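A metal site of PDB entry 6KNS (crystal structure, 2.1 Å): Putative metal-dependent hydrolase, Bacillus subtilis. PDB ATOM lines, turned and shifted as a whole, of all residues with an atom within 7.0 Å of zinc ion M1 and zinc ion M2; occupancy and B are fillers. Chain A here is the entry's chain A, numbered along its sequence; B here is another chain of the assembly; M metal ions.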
ATOM      1  N   TYR A  15      27.196   2.070 -27.595  1.00  0.00           N
ATOM      2  CA  TYR A  15      27.318   0.632 -27.864  1.00  0.00           C
ATOM      3  C   TYR A  15      27.016  -0.275 -26.688  1.00  0.00           C
ATOM      4  O   TYR A  15      27.349   0.033 -25.536  1.00  0.00           O
ATOM      5  CB  TYR A  15      28.698   0.277 -28.460  1.00  0.00           C
ATOM      6  CG  TYR A  15      28.740   0.554 -29.951  1.00  0.00           C
ATOM      7  CD1 TYR A  15      28.397  -0.428 -30.873  1.00  0.00           C
ATOM      8  CD2 TYR A  15      29.064   1.805 -30.426  1.00  0.00           C
ATOM      9  CE1 TYR A  15      28.372  -0.154 -32.220  1.00  0.00           C
ATOM     10  CE2 TYR A  15      29.054   2.099 -31.771  1.00  0.00           C
ATOM     11  CZ  TYR A  15      28.692   1.113 -32.661  1.00  0.00           C
ATOM     12  OH  TYR A  15      28.732   1.398 -33.995  1.00  0.00           O
ATOM     13  N   GLY A  16      26.414  -1.424 -26.984  1.00  0.00           N
ATOM     14  CA  GLY A  16      26.140  -2.402 -25.955  1.00  0.00           C
ATOM     15  C   GLY A  16      27.386  -3.249 -25.723  1.00  0.00           C
ATOM     16  O   GLY A  16      28.040  -3.606 -26.669  1.00  0.00           O
ATOM     17  N   GLY A  17      27.695  -3.566 -24.467  1.00  0.00           N
ATOM     18  CA  GLY A  17      28.721  -4.539 -24.101  1.00  0.00           C
ATOM     19  C   GLY A  17      30.153  -3.999 -24.061  1.00  0.00           C
ATOM     20  O   GLY A  17      30.819  -4.077 -23.020  1.00  0.00           O
ATOM     21  N   SER A  26      27.623   2.789 -22.910  1.00  0.00           N
ATOM     22  CA  SER A  26      26.630   3.681 -22.341  1.00  0.00           C
ATOM     23  C   SER A  26      27.130   4.865 -21.513  1.00  0.00           C
ATOM     24  O   SER A  26      27.827   4.707 -20.531  1.00  0.00           O
ATOM     25  CB  SER A  26      25.623   2.907 -21.524  1.00  0.00           C
ATOM     26  OG  SER A  26      24.923   1.959 -22.332  1.00  0.00           O
ATOM     27  N   ASP A  40      25.017   6.984 -16.522  1.00  0.00           N
ATOM     28  CA  ASP A  40      25.917   5.875 -16.869  1.00  0.00           C
ATOM     29  C   ASP A  40      27.267   6.381 -17.308  1.00  0.00           C
ATOM     30  O   ASP A  40      27.407   7.514 -17.806  1.00  0.00           O
ATOM     31  CB  ASP A  40      25.283   4.850 -17.849  1.00  0.00           C
ATOM     32  CG  ASP A  40      24.191   4.004 -17.168  1.00  0.00           C
ATOM     33  OD1 ASP A  40      24.094   4.054 -15.928  1.00  0.00           O
ATOM     34  OD2 ASP A  40      23.426   3.313 -17.835  1.00  0.00           O
ATOM     35  N   SER A  64      22.541   3.210 -13.839  1.00  0.00           N
ATOM     36  CA  SER A  64      21.349   2.355 -13.945  1.00  0.00           C
ATOM     37  C   SER A  64      21.636   0.965 -13.326  1.00  0.00           C
ATOM     38  O   SER A  64      20.736   0.371 -12.716  1.00  0.00           O
ATOM     39  CB  SER A  64      20.955   2.148 -15.394  1.00  0.00           C
ATOM     40  OG  SER A  64      22.057   1.608 -16.135  1.00  0.00           O
ATOM     41  N   HIS A  65      22.847   0.475 -13.514  1.00  0.00           N
ATOM     42  CA  HIS A  65      23.253  -0.829 -13.018  1.00  0.00           C
ATOM     43  C   HIS A  65      24.762  -0.998 -13.128  1.00  0.00           C
ATOM     44  O   HIS A  65      25.445  -0.124 -13.681  1.00  0.00           O
ATOM     45  CB  HIS A  65      22.494  -1.953 -13.718  1.00  0.00           C
ATOM     46  CG  HIS A  65      22.847  -2.184 -15.162  1.00  0.00           C
ATOM     47  ND1 HIS A  65      22.639  -1.243 -16.159  1.00  0.00           N
ATOM     48  CD2 HIS A  65      23.264  -3.315 -15.800  1.00  0.00           C
ATOM     49  CE1 HIS A  65      22.949  -1.788 -17.330  1.00  0.00           C
ATOM     50  NE2 HIS A  65      23.334  -3.032 -17.143  1.00  0.00           N
ATOM     51  N   TYR A  66      25.278  -2.106 -12.604  1.00  0.00           N
ATOM     52  CA  TYR A  66      26.704  -2.245 -12.444  1.00  0.00           C
ATOM     53  C   TYR A  66      27.410  -3.186 -13.417  1.00  0.00           C
ATOM     54  O   TYR A  66      28.532  -3.619 -13.166  1.00  0.00           O
ATOM     55  CB  TYR A  66      26.997  -2.664 -11.005  1.00  0.00           C
ATOM     56  CG  TYR A  66      26.497  -1.654  -9.942  1.00  0.00           C
ATOM     57  CD1 TYR A  66      27.158  -0.456  -9.763  1.00  0.00           C
ATOM     58  CD2 TYR A  66      25.418  -1.917  -9.145  1.00  0.00           C
ATOM     59  CE1 TYR A  66      26.763   0.457  -8.821  1.00  0.00           C
ATOM     60  CE2 TYR A  66      25.001  -0.980  -8.155  1.00  0.00           C
ATOM     61  CZ  TYR A  66      25.677   0.204  -8.018  1.00  0.00           C
ATOM     62  OH  TYR A  66      25.365   1.163  -7.086  1.00  0.00           O
ATOM     63  N   HIS A  67      26.803  -3.436 -14.562  1.00  0.00           N
ATOM     64  CA  HIS A  67      27.488  -4.141 -15.663  1.00  0.00           C
ATOM     65  C   HIS A  67      28.643  -3.243 -16.150  1.00  0.00           C
ATOM     66  O   HIS A  67      28.507  -2.020 -16.183  1.00  0.00           O
ATOM     67  CB  HIS A  67      26.496  -4.407 -16.811  1.00  0.00           C
ATOM     68  CG  HIS A  67      25.789  -5.715 -16.745  1.00  0.00           C
ATOM     69  ND1 HIS A  67      24.659  -5.989 -17.486  1.00  0.00           N
ATOM     70  CD2 HIS A  67      26.103  -6.874 -16.097  1.00  0.00           C
ATOM     71  CE1 HIS A  67      24.281  -7.242 -17.267  1.00  0.00           C
ATOM     72  NE2 HIS A  67      25.143  -7.797 -16.421  1.00  0.00           N
ATOM     73  N   HIS A  68      29.760  -3.872 -16.554  1.00  0.00           N
ATOM     74  CA  HIS A  68      30.992  -3.177 -16.971  1.00  0.00           C
ATOM     75  C   HIS A  68      30.779  -2.084 -17.992  1.00  0.00           C
ATOM     76  O   HIS A  68      31.350  -0.984 -17.907  1.00  0.00           O
ATOM     77  CB  HIS A  68      31.982  -4.160 -17.585  1.00  0.00           C
ATOM     78  CG  HIS A  68      32.436  -5.214 -16.668  1.00  0.00           C
ATOM     79  ND1 HIS A  68      33.031  -4.942 -15.440  1.00  0.00           N
ATOM     80  CD2 HIS A  68      32.378  -6.573 -16.777  1.00  0.00           C
ATOM     81  CE1 HIS A  68      33.334  -6.091 -14.858  1.00  0.00           C
ATOM     82  NE2 HIS A  68      32.942  -7.089 -15.642  1.00  0.00           N
ATOM     83  N   ASP A  69      29.946  -2.363 -18.978  1.00  0.00           N
ATOM     84  CA  ASP A  69      29.668  -1.364 -20.017  1.00  0.00           C
ATOM     85  C   ASP A  69      28.876  -0.130 -19.568  1.00  0.00           C
ATOM     86  O   ASP A  69      28.698   0.807 -20.364  1.00  0.00           O
ATOM     87  CB  ASP A  69      29.059  -2.030 -21.255  1.00  0.00           C
ATOM     88  CG  ASP A  69      27.716  -2.690 -20.959  1.00  0.00           C
ATOM     89  OD1 ASP A  69      27.643  -3.386 -19.957  1.00  0.00           O
ATOM     90  OD2 ASP A  69      26.778  -2.506 -21.749  1.00  0.00           O
ATOM     91  N   HIS A  70      28.470  -0.085 -18.305  1.00  0.00           N
ATOM     92  CA  HIS A  70      27.838   1.105 -17.724  1.00  0.00           C
ATOM     93  C   HIS A  70      28.641   1.782 -16.600  1.00  0.00           C
ATOM     94  O   HIS A  70      28.255   2.863 -16.144  1.00  0.00           O
ATOM     95  CB  HIS A  70      26.439   0.718 -17.204  1.00  0.00           C
ATOM     96  CG  HIS A  70      25.544   0.253 -18.312  1.00  0.00           C
ATOM     97  ND1 HIS A  70      24.502   1.015 -18.800  1.00  0.00           N
ATOM     98  CD2 HIS A  70      25.610  -0.856 -19.080  1.00  0.00           C
ATOM     99  CE1 HIS A  70      23.956   0.357 -19.814  1.00  0.00           C
ATOM    100  NE2 HIS A  70      24.598  -0.785 -19.985  1.00  0.00           N
ATOM    101  N   HIS A 140      16.452  -7.896 -16.240  1.00  0.00           N
ATOM    102  CA  HIS A 140      17.843  -7.942 -16.676  1.00  0.00           C
ATOM    103  C   HIS A 140      18.632  -8.927 -15.798  1.00  0.00           C
ATOM    104  O   HIS A 140      18.211  -9.210 -14.682  1.00  0.00           O
ATOM    105  CB  HIS A 140      18.419  -6.523 -16.593  1.00  0.00           C
ATOM    106  CG  HIS A 140      19.607  -6.308 -17.456  1.00  0.00           C
ATOM    107  ND1 HIS A 140      19.591  -6.587 -18.804  1.00  0.00           N
ATOM    108  CD2 HIS A 140      20.852  -5.858 -17.184  1.00  0.00           C
ATOM    109  CE1 HIS A 140      20.768  -6.312 -19.323  1.00  0.00           C
ATOM    110  NE2 HIS A 140      21.548  -5.868 -18.359  1.00  0.00           N
ATOM    111  N   PRO A 141      19.736  -9.507 -16.291  1.00  0.00           N
ATOM    112  CA  PRO A 141      20.387 -10.502 -15.434  1.00  0.00           C
ATOM    113  C   PRO A 141      21.019  -9.960 -14.164  1.00  0.00           C
ATOM    114  O   PRO A 141      21.428 -10.755 -13.362  1.00  0.00           O
ATOM    115  CB  PRO A 141      21.475 -11.114 -16.339  1.00  0.00           C
ATOM    116  CG  PRO A 141      21.252 -10.590 -17.704  1.00  0.00           C
ATOM    117  CD  PRO A 141      20.306  -9.454 -17.641  1.00  0.00           C
ATOM    118  N   VAL A 142      21.223  -8.641 -14.017  1.00  0.00           N
ATOM    119  CA  VAL A 142      21.544  -8.029 -12.725  1.00  0.00           C
ATOM    120  C   VAL A 142      20.510  -6.953 -12.459  1.00  0.00           C
ATOM    121  O   VAL A 142      19.814  -6.511 -13.370  1.00  0.00           O
ATOM    122  CB  VAL A 142      22.965  -7.407 -12.658  1.00  0.00           C
ATOM    123  CG1 VAL A 142      24.064  -8.501 -12.773  1.00  0.00           C
ATOM    124  CG2 VAL A 142      23.174  -6.274 -13.691  1.00  0.00           C
ATOM    125  N   CYS A 144      18.716  -3.698 -12.228  1.00  0.00           N
ATOM    126  CA  CYS A 144      18.903  -2.558 -13.094  1.00  0.00           C
ATOM    127  C   CYS A 144      17.677  -1.682 -13.022  1.00  0.00           C
ATOM    128  O   CYS A 144      16.565  -2.219 -12.861  1.00  0.00           O
ATOM    129  CB  CYS A 144      19.229  -3.027 -14.537  1.00  0.00           C
ATOM    130  SG  CYS A 144      19.411  -1.685 -15.692  1.00  0.00           S
ATOM    131  N   TYR A 158      14.757   6.879 -20.064  1.00  0.00           N
ATOM    132  CA  TYR A 158      15.881   6.015 -20.412  1.00  0.00           C
ATOM    133  C   TYR A 158      15.545   4.623 -19.885  1.00  0.00           C
ATOM    134  O   TYR A 158      15.341   4.454 -18.698  1.00  0.00           O
ATOM    135  CB  TYR A 158      17.138   6.519 -19.702  1.00  0.00           C
ATOM    136  CG  TYR A 158      18.361   5.686 -19.819  1.00  0.00           C
ATOM    137  CD1 TYR A 158      18.786   5.203 -21.058  1.00  0.00           C
ATOM    138  CD2 TYR A 158      19.158   5.405 -18.690  1.00  0.00           C
ATOM    139  CE1 TYR A 158      19.984   4.436 -21.172  1.00  0.00           C
ATOM    140  CE2 TYR A 158      20.342   4.659 -18.793  1.00  0.00           C
ATOM    141  CZ  TYR A 158      20.749   4.189 -20.025  1.00  0.00           C
ATOM    142  OH  TYR A 158      21.905   3.460 -20.143  1.00  0.00           O
ATOM    143  N   ALA A 160      17.471   2.124 -19.641  1.00  0.00           N
ATOM    144  CA  ALA A 160      18.628   1.350 -19.278  1.00  0.00           C
ATOM    145  C   ALA A 160      18.539   0.027 -20.066  1.00  0.00           C
ATOM    146  O   ALA A 160      18.081   0.014 -21.224  1.00  0.00           O
ATOM    147  CB  ALA A 160      18.704   1.125 -17.765  1.00  0.00           C
ATOM    148  N   ASP A 161      18.967  -1.077 -19.455  1.00  0.00           N
ATOM    149  CA  ASP A 161      18.931  -2.372 -20.102  1.00  0.00           C
ATOM    150  C   ASP A 161      17.751  -3.162 -19.620  1.00  0.00           C
ATOM    151  O   ASP A 161      17.550  -3.282 -18.415  1.00  0.00           O
ATOM    152  CB  ASP A 161      20.152  -3.181 -19.731  1.00  0.00           C
ATOM    153  CG  ASP A 161      21.427  -2.655 -20.355  1.00  0.00           C
ATOM    154  OD1 ASP A 161      21.497  -1.507 -20.885  1.00  0.00           O
ATOM    155  OD2 ASP A 161      22.347  -3.451 -20.328  1.00  0.00           O
ATOM    156  N   SER A 162      17.026  -3.772 -20.540  1.00  0.00           N
ATOM    157  CA  SER A 162      15.888  -4.622 -20.151  1.00  0.00           C
ATOM    158  C   SER A 162      15.413  -5.468 -21.322  1.00  0.00           C
ATOM    159  O   SER A 162      15.542  -5.066 -22.478  1.00  0.00           O
ATOM    160  CB  SER A 162      14.733  -3.737 -19.710  1.00  0.00           C
ATOM    161  OG  SER A 162      13.682  -4.483 -19.105  1.00  0.00           O
ATOM    162  N   GLU A 181      17.070   0.987 -25.140  1.00  0.00           N
ATOM    163  CA  GLU A 181      18.030   0.013 -25.551  1.00  0.00           C
ATOM    164  C   GLU A 181      17.405  -0.728 -26.743  1.00  0.00           C
ATOM    165  O   GLU A 181      16.178  -0.831 -26.880  1.00  0.00           O
ATOM    166  CB  GLU A 181      18.386  -0.905 -24.370  1.00  0.00           C
ATOM    167  CG  GLU A 181      17.419  -2.020 -24.021  1.00  0.00           C
ATOM    168  CD  GLU A 181      18.112  -3.385 -24.136  1.00  0.00           C
ATOM    169  OE1 GLU A 181      18.160  -3.953 -25.255  1.00  0.00           O
ATOM    170  OE2 GLU A 181      18.642  -3.855 -23.094  1.00  0.00           O
ATOM    171  N   ASN A 183      19.347  -3.774 -28.462  1.00  0.00           N
ATOM    172  CA  ASN A 183      20.534  -4.560 -28.730  1.00  0.00           C
ATOM    173  C   ASN A 183      20.294  -5.645 -29.801  1.00  0.00           C
ATOM    174  O   ASN A 183      21.256  -6.216 -30.267  1.00  0.00           O
ATOM    175  CB  ASN A 183      21.019  -5.221 -27.434  1.00  0.00           C
ATOM    176  CG  ASN A 183      22.559  -5.336 -27.376  1.00  0.00           C
ATOM    177  OD1 ASN A 183      23.220  -5.653 -28.368  1.00  0.00           O
ATOM    178  ND2 ASN A 183      23.109  -5.066 -26.238  1.00  0.00           N
ATOM    179  N   ALA A 193      19.004 -12.755 -22.978  1.00  0.00           N
ATOM    180  CA  ALA A 193      20.084 -11.814 -22.618  1.00  0.00           C
ATOM    181  C   ALA A 193      19.620 -10.610 -21.810  1.00  0.00           C
ATOM    182  O   ALA A 193      20.442  -9.753 -21.459  1.00  0.00           O
ATOM    183  CB  ALA A 193      20.832 -11.340 -23.900  1.00  0.00           C
ATOM    184  N   GLY A 194      18.335 -10.480 -21.547  1.00  0.00           N
ATOM    185  CA  GLY A 194      17.832  -9.288 -20.856  1.00  0.00           C
ATOM    186  C   GLY A 194      17.869  -8.008 -21.686  1.00  0.00           C
ATOM    187  O   GLY A 194      18.131  -6.904 -21.159  1.00  0.00           O
ATOM    188  N   HIS A 195      17.609  -8.163 -22.971  1.00  0.00           N
ATOM    189  CA  HIS A 195      17.593  -7.038 -23.916  1.00  0.00           C
ATOM    190  C   HIS A 195      16.334  -7.012 -24.780  1.00  0.00           C
ATOM    191  O   HIS A 195      15.540  -7.943 -24.807  1.00  0.00           O
ATOM    192  CB  HIS A 195      18.821  -7.068 -24.833  1.00  0.00           C
ATOM    193  CG  HIS A 195      20.113  -6.846 -24.118  1.00  0.00           C
ATOM    194  ND1 HIS A 195      20.368  -5.730 -23.347  1.00  0.00           N
ATOM    195  CD2 HIS A 195      21.240  -7.598 -24.077  1.00  0.00           C
ATOM    196  CE1 HIS A 195      21.598  -5.801 -22.869  1.00  0.00           C
ATOM    197  NE2 HIS A 195      22.137  -6.941 -23.263  1.00  0.00           N
ATOM    198  N   HIS A 217      22.350   1.300 -27.186  1.00  0.00           N
ATOM    199  CA  HIS A 217      22.896   0.027 -26.703  1.00  0.00           C
ATOM    200  C   HIS A 217      23.023  -0.928 -27.865  1.00  0.00           C
ATOM    201  O   HIS A 217      22.583  -2.070 -27.809  1.00  0.00           O
ATOM    202  CB  HIS A 217      22.022  -0.550 -25.606  1.00  0.00           C
ATOM    203  CG  HIS A 217      22.762  -1.372 -24.620  1.00  0.00           C
ATOM    204  ND1 HIS A 217      23.013  -2.720 -24.819  1.00  0.00           N
ATOM    205  CD2 HIS A 217      23.341  -1.034 -23.447  1.00  0.00           C
ATOM    206  CE1 HIS A 217      23.679  -3.183 -23.770  1.00  0.00           C
ATOM    207  NE2 HIS A 217      23.900  -2.176 -22.928  1.00  0.00           N
ATOM    208  N   PHE B  79      33.547  -8.592 -21.771  1.00  0.00           N
ATOM    209  CA  PHE B  79      32.327  -8.635 -22.544  1.00  0.00           C
ATOM    210  C   PHE B  79      32.593  -8.744 -24.064  1.00  0.00           C
ATOM    211  O   PHE B  79      31.849  -9.429 -24.748  1.00  0.00           O
ATOM    212  CB  PHE B  79      31.445  -7.449 -22.229  1.00  0.00           C
ATOM    213  CG  PHE B  79      30.748  -7.517 -20.878  1.00  0.00           C
ATOM    214  CD1 PHE B  79      30.780  -8.677 -20.072  1.00  0.00           C
ATOM    215  CD2 PHE B  79      29.970  -6.432 -20.450  1.00  0.00           C
ATOM    216  CE1 PHE B  79      30.104  -8.719 -18.845  1.00  0.00           C
ATOM    217  CE2 PHE B  79      29.281  -6.485 -19.219  1.00  0.00           C
ATOM    218  CZ  PHE B  79      29.347  -7.634 -18.426  1.00  0.00           C
HETATM  219 ZN    ZN M   1      24.389  -2.732 -20.950  1.00  0.00          ZN
HETATM  220 ZN    ZN M   2      23.467  -4.702 -18.657  1.00  0.00          ZN
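Five residues have an atom within 4 Å of zinc ion M1: His 65, Asp 69, His 70, Asp 161 and His 217.
The nearest printed residue that does not touch zinc ion M1 is His 195 (4.6 Å).
Zinc ion M1 is bound by a ring nitrogen (NE2) of His 217 (2.1 Å), a ring nitrogen (NE2) of His 70 (2.2 Å), the side-chain carboxylate (OD2) of Asp 161 (2.3 Å) and the side-chain carboxylate (OD2) of Asp 69 (2.5 Å).
Four residues have an atom within 4 Å of zinc ion M2: His 65, His 67, His 140 and Asp 161.
The nearest printed residue that does not touch zinc ion M2 is His 70 (4.3 Å).
ND1 of His 217 lies within hydrogen-bond range of ND2 of Asn 183, 2.7 Å away.
A ring nitrogen (ND1) of His 70 is in hydrogen-bond range of the side-chain carboxylate of Asp 40 (2.7 Å).
SG of Cys 144 sits at hydrogen-bond distance from O of Asp 161 (3.7 Å).
A ring nitrogen (ND1) of His 65 lies within hydrogen-bond range of the side-chain sulfur (SG) of Cys 144, 3.3 Å away.
ND1 of His 65 lies within hydrogen-bond range of OG of Ser 64, 2.9 Å away.
ND1 of His 140 lies within hydrogen-bond range of O of Gly 194, 2.8 Å away.
The side-chain carboxylate (OD2) of Asp 69 lies close to the backbone NH (N) of Gly 17.
N of Ser 26 is in hydrogen-bond range of O of Asp 69, at 3.4 Å.
ND1 of His 67 is bound to zinc ion M2 (2.1 Å).
Zinc ion M2 is bound by NE2 of His 65, at 2.3 Å.
A ring nitrogen (NE2) of His 140 is bound to zinc ion M2 (2.3 Å).
OD2 of Asp 161 binds zinc ion M2.
Zinc ion M2 has four donor atoms within binding distance.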
